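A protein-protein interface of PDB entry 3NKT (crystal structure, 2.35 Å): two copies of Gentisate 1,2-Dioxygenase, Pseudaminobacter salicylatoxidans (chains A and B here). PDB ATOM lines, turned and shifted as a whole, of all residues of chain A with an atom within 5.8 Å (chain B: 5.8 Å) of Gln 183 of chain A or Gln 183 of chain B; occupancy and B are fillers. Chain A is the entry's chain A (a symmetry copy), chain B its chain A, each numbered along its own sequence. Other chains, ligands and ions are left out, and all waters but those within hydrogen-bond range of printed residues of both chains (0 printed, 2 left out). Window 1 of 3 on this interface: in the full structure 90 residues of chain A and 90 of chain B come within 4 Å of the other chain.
The backbone NH (N) of Phe 180 of chain B is in hydrogen-bond range of the backbone carbonyl oxygen (O) of Thr 102 of chain B (3.1 Å).
The backbone carbonyl oxygen (O) of Thr 102 of chain A lies within hydrogen-bond range of the backbone NH (N) of Phe 180 of chain A (3.1 Å).
The backbone carbonyl oxygen of Pro 179 of chain A sits close to the side-chain amide oxygen of Gln 183 of chain A, at 2.9 Å.
O of Pro 101 of chain A sits close to OE1 of Gln 183 of chain A, 2.7 Å away.
The side-chain amide oxygen (OE1) of Gln 183 of chain B sits close to the backbone carbonyl oxygen (O) of Pro 179 of chain B (2.9 Å).
The side-chain amide oxygen (OE1) of Gln 183 of chain B lies close to the backbone carbonyl oxygen (O) of Pro 101 of chain B.
Among the printed residues, merely in contact across the chains: Pro 101 of chain A with Gln 183 of chain B (3.2 Å), Gln 183 of chain A with Pro 101 of chain B (3.2 Å), Pro 101 of chain A with Asp 185 of chain B (3.3 Å), Asp 185 of chain A with Pro 101 of chain B (3.3 Å), Thr 102 of chain A with Met 184 of chain B (3.6 Å), Met 184 of chain A with Thr 102 of chain B (3.6 Å), Phe 180 of chain A with Phe 180 of chain B (3.6 Å), Met 184 of chain A with Phe 180 of chain B (3.7 Å), Phe 180 of chain A with Met 184 of chain B (3.7 Å), Met 184 of chain A with Gln 183 of chain B (3.7 Å), Gln 183 of chain A with Met 184 of chain B (3.7 Å), Pro 101 of chain A with Met 184 of chain B (3.8 Å), Met 184 of chain A with Pro 101 of chain B (3.8 Å) and Gln 183 of chain A with Gln 183 of chain B (3.9 Å).
Of chain B, only Pro 101 (3.2 Å), Gln 183 (3.9 Å) and Met 184 (3.7 Å) come within 4 Å of Gln 183 of chain A.
Of chain A, only Pro 101, Gln 183 and Met 184 come within 4 Å of Gln 183 of chain B.
Printed residues of chain A within 4 Å of Met 184 of chain B: Pro 101 (3.8 Å), Thr 102 (3.6 Å), Phe 180 (3.7 Å) and Gln 183 (3.7 Å).
Printed residues of chain B within 4 Å of Pro 101 of chain A: Gln 183, Met 184 and Asp 185.
Of the printed residues of chain B, Asp 185 of chain A touches Pro 101 (3.3 Å).
Ile 178 of chain B touches none of the printed residues of chain A.
Hydrophobic or aromatic side chains of chain A within 4 Å of the printed part of chain B: Pro 101, Phe 180 and Met 184.
Printed residues of chain B that touch a printed residue of chain A: Pro 101, Thr 102, Phe 180, Gln 183, Met 184 and Asp 185.
Hydrophobic or aromatic side chains of chain B that line the printed part of chain A: Pro 101, Phe 180 and Met 184.
Among the printed residues, no Asp or Glu carboxylate lies within 4 Å of a Lys or Arg side-chain nitrogen of the other chain.
Pro 101 of chain A touches Gln 183 of chain B, and with the chains exchanged Gln 183 of chain A touches Pro 101 of chain B.
Pro 101 of chain A touches Met 184 of chain B, and with the chains exchanged Met 184 of chain A touches Pro 101 of chain B.
Pro 101 of chain A touches Asp 185 of chain B, and with the chains exchanged Asp 185 of chain A touches Pro 101 of chain B.
Phe 180 of chain A touches Met 184 of chain B, and with the chains exchanged Met 184 of chain A touches Phe 180 of chain B.
Positions printed for both chains: 98, 101, 102, 178, 179, 180, 181, 182, 183, 184 and 185.
Of the 14 pairs that touch across the chains among the printed residues, 14 have their exchanged pair printed and touching as well.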
ATOM      1  N   TYR A  98     -10.580  20.259  28.768  1.00  0.00           N
ATOM      2  CA  TYR A  98     -10.826  20.047  27.330  1.00  0.00           C
ATOM      3  C   TYR A  98     -10.504  21.308  26.573  1.00  0.00           C
ATOM      4  O   TYR A  98     -11.082  22.339  26.932  1.00  0.00           O
ATOM      5  CB  TYR A  98     -12.316  19.885  27.121  1.00  0.00           C
ATOM      6  CG  TYR A  98     -13.007  18.713  27.756  1.00  0.00           C
ATOM      7  CD1 TYR A  98     -12.309  17.701  28.394  1.00  0.00           C
ATOM      8  CD2 TYR A  98     -14.375  18.605  27.660  1.00  0.00           C
ATOM      9  CE1 TYR A  98     -12.961  16.627  28.935  1.00  0.00           C
ATOM     10  CE2 TYR A  98     -15.038  17.535  28.170  1.00  0.00           C
ATOM     11  CZ  TYR A  98     -14.332  16.552  28.813  1.00  0.00           C
ATOM     12  OH  TYR A  98     -15.020  15.499  29.343  1.00  0.00           O
ATOM     13  N   PRO A 101     -14.638  20.344  22.726  1.00  0.00           N
ATOM     14  CA  PRO A 101     -15.453  19.185  23.164  1.00  0.00           C
ATOM     15  C   PRO A 101     -14.867  17.813  22.778  1.00  0.00           C
ATOM     16  O   PRO A 101     -15.263  16.798  23.341  1.00  0.00           O
ATOM     17  CB  PRO A 101     -16.786  19.399  22.442  1.00  0.00           C
ATOM     18  CG  PRO A 101     -16.809  20.871  22.147  1.00  0.00           C
ATOM     19  CD  PRO A 101     -15.382  21.215  21.801  1.00  0.00           C
ATOM     20  N   THR A 102     -13.934  17.793  21.834  1.00  0.00           N
ATOM     21  CA  THR A 102     -13.389  16.516  21.371  1.00  0.00           C
ATOM     22  C   THR A 102     -11.952  16.257  21.802  1.00  0.00           C
ATOM     23  O   THR A 102     -11.519  15.112  21.840  1.00  0.00           O
ATOM     24  CB  THR A 102     -13.457  16.424  19.836  1.00  0.00           C
ATOM     25  OG1 THR A 102     -12.822  17.574  19.280  1.00  0.00           O
ATOM     26  CG2 THR A 102     -14.932  16.425  19.366  1.00  0.00           C
ATOM     27  N   ILE A 178      -9.036  12.331  24.225  1.00  0.00           N
ATOM     28  CA  ILE A 178      -9.445  12.263  25.643  1.00  0.00           C
ATOM     29  C   ILE A 178     -10.899  12.775  25.909  1.00  0.00           C
ATOM     30  O   ILE A 178     -11.696  12.027  26.464  1.00  0.00           O
ATOM     31  CB  ILE A 178      -8.385  12.967  26.598  1.00  0.00           C
ATOM     32  CG1 ILE A 178      -7.243  12.034  26.918  1.00  0.00           C
ATOM     33  CG2 ILE A 178      -9.032  13.439  27.920  1.00  0.00           C
ATOM     34  CD1 ILE A 178      -7.685  10.719  27.575  1.00  0.00           C
ATOM     35  N   PRO A 179     -11.236  14.024  25.503  1.00  0.00           N
ATOM     36  CA  PRO A 179     -12.605  14.574  25.740  1.00  0.00           C
ATOM     37  C   PRO A 179     -13.770  13.891  24.977  1.00  0.00           C
ATOM     38  O   PRO A 179     -14.828  13.601  25.583  1.00  0.00           O
ATOM     39  CB  PRO A 179     -12.476  16.058  25.317  1.00  0.00           C
ATOM     40  CG  PRO A 179     -11.042  16.348  25.478  1.00  0.00           C
ATOM     41  CD  PRO A 179     -10.338  15.083  25.018  1.00  0.00           C
ATOM     42  N   PHE A 180     -13.628  13.704  23.670  1.00  0.00           N
ATOM     43  CA  PHE A 180     -14.582  12.840  22.940  1.00  0.00           C
ATOM     44  C   PHE A 180     -14.720  11.510  23.691  1.00  0.00           C
ATOM     45  O   PHE A 180     -15.802  11.009  23.881  1.00  0.00           O
ATOM     46  CB  PHE A 180     -14.065  12.538  21.509  1.00  0.00           C
ATOM     47  CG  PHE A 180     -14.976  11.647  20.717  1.00  0.00           C
ATOM     48  CD1 PHE A 180     -14.789  10.254  20.699  1.00  0.00           C
ATOM     49  CD2 PHE A 180     -16.036  12.183  20.012  1.00  0.00           C
ATOM     50  CE1 PHE A 180     -15.639   9.427  19.996  1.00  0.00           C
ATOM     51  CE2 PHE A 180     -16.909  11.347  19.304  1.00  0.00           C
ATOM     52  CZ  PHE A 180     -16.695   9.969  19.285  1.00  0.00           C
ATOM     53  N   SER A 181     -13.592  10.944  24.109  1.00  0.00           N
ATOM     54  CA  SER A 181     -13.612   9.592  24.636  1.00  0.00           C
ATOM     55  C   SER A 181     -14.295   9.472  26.009  1.00  0.00           C
ATOM     56  O   SER A 181     -14.970   8.474  26.284  1.00  0.00           O
ATOM     57  CB  SER A 181     -12.195   9.025  24.706  1.00  0.00           C
ATOM     58  OG  SER A 181     -11.648   8.857  23.410  1.00  0.00           O
ATOM     59  N   GLN A 182     -14.088  10.475  26.864  1.00  0.00           N
ATOM     60  CA  GLN A 182     -14.789  10.553  28.133  1.00  0.00           C
ATOM     61  C   GLN A 182     -16.305  10.690  27.952  1.00  0.00           C
ATOM     62  O   GLN A 182     -17.061   9.940  28.548  1.00  0.00           O
ATOM     63  CB  GLN A 182     -14.231  11.695  29.012  1.00  0.00           C
ATOM     64  CG  GLN A 182     -15.089  12.027  30.250  1.00  0.00           C
ATOM     65  CD  GLN A 182     -14.304  12.830  31.268  1.00  0.00           C
ATOM     66  OE1 GLN A 182     -13.902  12.294  32.304  1.00  0.00           O
ATOM     67  NE2 GLN A 182     -14.030  14.107  30.958  1.00  0.00           N
ATOM     68  N   GLN A 183     -16.744  11.636  27.138  1.00  0.00           N
ATOM     69  CA  GLN A 183     -18.176  11.894  27.002  1.00  0.00           C
ATOM     70  C   GLN A 183     -18.844  10.765  26.290  1.00  0.00           C
ATOM     71  O   GLN A 183     -20.023  10.537  26.561  1.00  0.00           O
ATOM     72  CB  GLN A 183     -18.474  13.203  26.261  1.00  0.00           C
ATOM     73  CG  GLN A 183     -18.021  14.471  26.997  1.00  0.00           C
ATOM     74  CD  GLN A 183     -17.813  15.629  26.020  1.00  0.00           C
ATOM     75  OE1 GLN A 183     -16.868  15.621  25.216  1.00  0.00           O
ATOM     76  NE2 GLN A 183     -18.723  16.608  26.054  1.00  0.00           N
ATOM     77  N   MET A 184     -18.140  10.074  25.387  1.00  0.00           N
ATOM     78  CA  MET A 184     -18.733   8.944  24.643  1.00  0.00           C
ATOM     79  C   MET A 184     -18.630   7.544  25.293  1.00  0.00           C
ATOM     80  O   MET A 184     -19.210   6.557  24.775  1.00  0.00           O
ATOM     81  CB  MET A 184     -18.218   8.898  23.189  1.00  0.00           C
ATOM     82  CG  MET A 184     -18.544  10.173  22.382  1.00  0.00           C
ATOM     83  SD  MET A 184     -20.321  10.563  22.376  1.00  0.00           S
ATOM     84  CE  MET A 184     -20.616  11.839  23.528  1.00  0.00           C
ATOM     85  N   ASP A 185     -17.892   7.455  26.405  1.00  0.00           N
ATOM     86  CA  ASP A 185     -17.648   6.173  27.111  1.00  0.00           C
ATOM     87  C   ASP A 185     -16.881   5.103  26.314  1.00  0.00           C
ATOM     88  O   ASP A 185     -17.293   3.937  26.251  1.00  0.00           O
ATOM     89  CB  ASP A 185     -18.949   5.583  27.674  1.00  0.00           C
ATOM     90  CG  ASP A 185     -19.768   6.593  28.510  1.00  0.00           C
ATOM     91  OD1 ASP A 185     -19.199   7.285  29.396  1.00  0.00           O
ATOM     92  OD2 ASP A 185     -21.000   6.664  28.298  1.00  0.00           O
ATOM     93  N   TYR B  98     -31.227  13.400  27.717  1.00  0.00           N
ATOM     94  CA  TYR B  98     -30.460  12.372  26.991  1.00  0.00           C
ATOM     95  C   TYR B  98     -30.743  11.018  27.585  1.00  0.00           C
ATOM     96  O   TYR B  98     -30.544  10.887  28.797  1.00  0.00           O
ATOM     97  CB  TYR B  98     -28.990  12.582  27.283  1.00  0.00           C
ATOM     98  CG  TYR B  98     -28.343  13.862  26.835  1.00  0.00           C
ATOM     99  CD1 TYR B  98     -29.004  14.783  26.039  1.00  0.00           C
ATOM    100  CD2 TYR B  98     -27.036  14.111  27.180  1.00  0.00           C
ATOM    101  CE1 TYR B  98     -28.380  15.926  25.618  1.00  0.00           C
ATOM    102  CE2 TYR B  98     -26.393  15.229  26.752  1.00  0.00           C
ATOM    103  CZ  TYR B  98     -27.068  16.137  25.979  1.00  0.00           C
ATOM    104  OH  TYR B  98     -26.412  17.267  25.583  1.00  0.00           O
ATOM    105  N   PRO B 101     -25.425   9.171  26.524  1.00  0.00           N
ATOM    106  CA  PRO B 101     -24.600  10.305  26.044  1.00  0.00           C
ATOM    107  C   PRO B 101     -24.728  10.592  24.535  1.00  0.00           C
ATOM    108  O   PRO B 101     -24.359  11.671  24.084  1.00  0.00           O
ATOM    109  CB  PRO B 101     -23.170   9.862  26.365  1.00  0.00           C
ATOM    110  CG  PRO B 101     -23.340   8.848  27.458  1.00  0.00           C
ATOM    111  CD  PRO B 101     -24.594   8.096  27.093  1.00  0.00           C
ATOM    112  N   THR B 102     -25.251   9.637  23.776  1.00  0.00           N
ATOM    113  CA  THR B 102     -25.334   9.818  22.326  1.00  0.00           C
ATOM    114  C   THR B 102     -26.749  10.025  21.804  1.00  0.00           C
ATOM    115  O   THR B 102     -26.931  10.573  20.723  1.00  0.00           O
ATOM    116  CB  THR B 102     -24.719   8.612  21.594  1.00  0.00           C
ATOM    117  OG1 THR B 102     -25.337   7.420  22.077  1.00  0.00           O
ATOM    118  CG2 THR B 102     -23.205   8.517  21.900  1.00  0.00           C
ATOM    119  N   ILE B 178     -29.481  13.513  18.617  1.00  0.00           N
ATOM    120  CA  ILE B 178     -29.586  14.802  19.331  1.00  0.00           C
ATOM    121  C   ILE B 178     -28.449  15.043  20.377  1.00  0.00           C
ATOM    122  O   ILE B 178     -27.763  16.054  20.282  1.00  0.00           O
ATOM    123  CB  ILE B 178     -31.030  15.010  19.967  1.00  0.00           C
ATOM    124  CG1 ILE B 178     -32.002  15.538  18.940  1.00  0.00           C
ATOM    125  CG2 ILE B 178     -30.992  15.983  21.167  1.00  0.00           C
ATOM    126  CD1 ILE B 178     -31.563  16.862  18.298  1.00  0.00           C
ATOM    127  N   PRO B 179     -28.248  14.116  21.347  1.00  0.00           N
ATOM    128  CA  PRO B 179     -27.186  14.295  22.383  1.00  0.00           C
ATOM    129  C   PRO B 179     -25.717  14.256  21.886  1.00  0.00           C
ATOM    130  O   PRO B 179     -24.901  15.121  22.283  1.00  0.00           O
ATOM    131  CB  PRO B 179     -27.453  13.138  23.377  1.00  0.00           C
ATOM    132  CG  PRO B 179     -28.880  12.833  23.188  1.00  0.00           C
ATOM    133  CD  PRO B 179     -29.113  12.978  21.695  1.00  0.00           C
ATOM    134  N   PHE B 180     -25.355  13.247  21.103  1.00  0.00           N
ATOM    135  CA  PHE B 180     -24.054  13.288  20.398  1.00  0.00           C
ATOM    136  C   PHE B 180     -23.925  14.637  19.680  1.00  0.00           C
ATOM    137  O   PHE B 180     -22.900  15.274  19.727  1.00  0.00           O
ATOM    138  CB  PHE B 180     -23.970  12.162  19.335  1.00  0.00           C
ATOM    139  CG  PHE B 180     -22.682  12.159  18.565  1.00  0.00           C
ATOM    140  CD1 PHE B 180     -22.570  12.841  17.342  1.00  0.00           C
ATOM    141  CD2 PHE B 180     -21.573  11.505  19.065  1.00  0.00           C
ATOM    142  CE1 PHE B 180     -21.382  12.864  16.642  1.00  0.00           C
ATOM    143  CE2 PHE B 180     -20.360  11.534  18.365  1.00  0.00           C
ATOM    144  CZ  PHE B 180     -20.275  12.202  17.142  1.00  0.00           C
ATOM    145  N   SER B 181     -24.990  15.056  19.005  1.00  0.00           N
ATOM    146  CA  SER B 181     -24.886  16.207  18.128  1.00  0.00           C
ATOM    147  C   SER B 181     -24.715  17.542  18.874  1.00  0.00           C
ATOM    148  O   SER B 181     -23.993  18.428  18.406  1.00  0.00           O
ATOM    149  CB  SER B 181     -26.096  16.281  17.197  1.00  0.00           C
ATOM    150  OG  SER B 181     -26.112  15.190  16.294  1.00  0.00           O
ATOM    151  N   GLN B 182     -25.401  17.678  20.009  1.00  0.00           N
ATOM    152  CA  GLN B 182     -25.217  18.825  20.880  1.00  0.00           C
ATOM    153  C   GLN B 182     -23.792  18.906  21.441  1.00  0.00           C
ATOM    154  O   GLN B 182     -23.157  19.944  21.347  1.00  0.00           O
ATOM    155  CB  GLN B 182     -26.261  18.839  22.019  1.00  0.00           C
ATOM    156  CG  GLN B 182     -25.972  19.859  23.140  1.00  0.00           C
ATOM    157  CD  GLN B 182     -27.205  20.120  23.981  1.00  0.00           C
ATOM    158  OE1 GLN B 182     -27.828  21.179  23.856  1.00  0.00           O
ATOM    159  NE2 GLN B 182     -27.603  19.138  24.803  1.00  0.00           N
ATOM    160  N   GLN B 183     -23.295  17.823  22.014  1.00  0.00           N
ATOM    161  CA  GLN B 183     -21.987  17.860  22.666  1.00  0.00           C
ATOM    162  C   GLN B 183     -20.903  17.999  21.651  1.00  0.00           C
ATOM    163  O   GLN B 183     -19.871  18.579  21.991  1.00  0.00           O
ATOM    164  CB  GLN B 183     -21.717  16.618  23.523  1.00  0.00           C
ATOM    165  CG  GLN B 183     -22.641  16.467  24.739  1.00  0.00           C
ATOM    166  CD  GLN B 183     -22.723  15.009  25.191  1.00  0.00           C
ATOM    167  OE1 GLN B 183     -23.307  14.160  24.500  1.00  0.00           O
ATOM    168  NE2 GLN B 183     -22.096  14.703  26.332  1.00  0.00           N
ATOM    169  N   MET B 184     -21.095  17.476  20.434  1.00  0.00           N
ATOM    170  CA  MET B 184     -20.069  17.575  19.377  1.00  0.00           C
ATOM    171  C   MET B 184     -20.109  18.830  18.472  1.00  0.00           C
ATOM    172  O   MET B 184     -19.201  19.037  17.629  1.00  0.00           O
ATOM    173  CB  MET B 184     -20.025  16.295  18.516  1.00  0.00           C
ATOM    174  CG  MET B 184     -19.699  15.023  19.326  1.00  0.00           C
ATOM    175  SD  MET B 184     -18.147  15.166  20.264  1.00  0.00           S
ATOM    176  CE  MET B 184     -18.532  15.505  21.931  1.00  0.00           C
ATOM    177  N   ASP B 185     -21.155  19.648  18.634  1.00  0.00           N
ATOM    178  CA  ASP B 185     -21.369  20.858  17.803  1.00  0.00           C
ATOM    179  C   ASP B 185     -21.580  20.610  16.298  1.00  0.00           C
ATOM    180  O   ASP B 185     -20.949  21.254  15.451  1.00  0.00           O
ATOM    181  CB  ASP B 185     -20.255  21.893  18.017  1.00  0.00           C
ATOM    182  CG  ASP B 185     -19.997  22.215  19.507  1.00  0.00           C
ATOM    183  OD1 ASP B 185     -20.964  22.470  20.273  1.00  0.00           O
ATOM    184  OD2 ASP B 185     -18.809  22.248  19.900  1.00  0.00           O
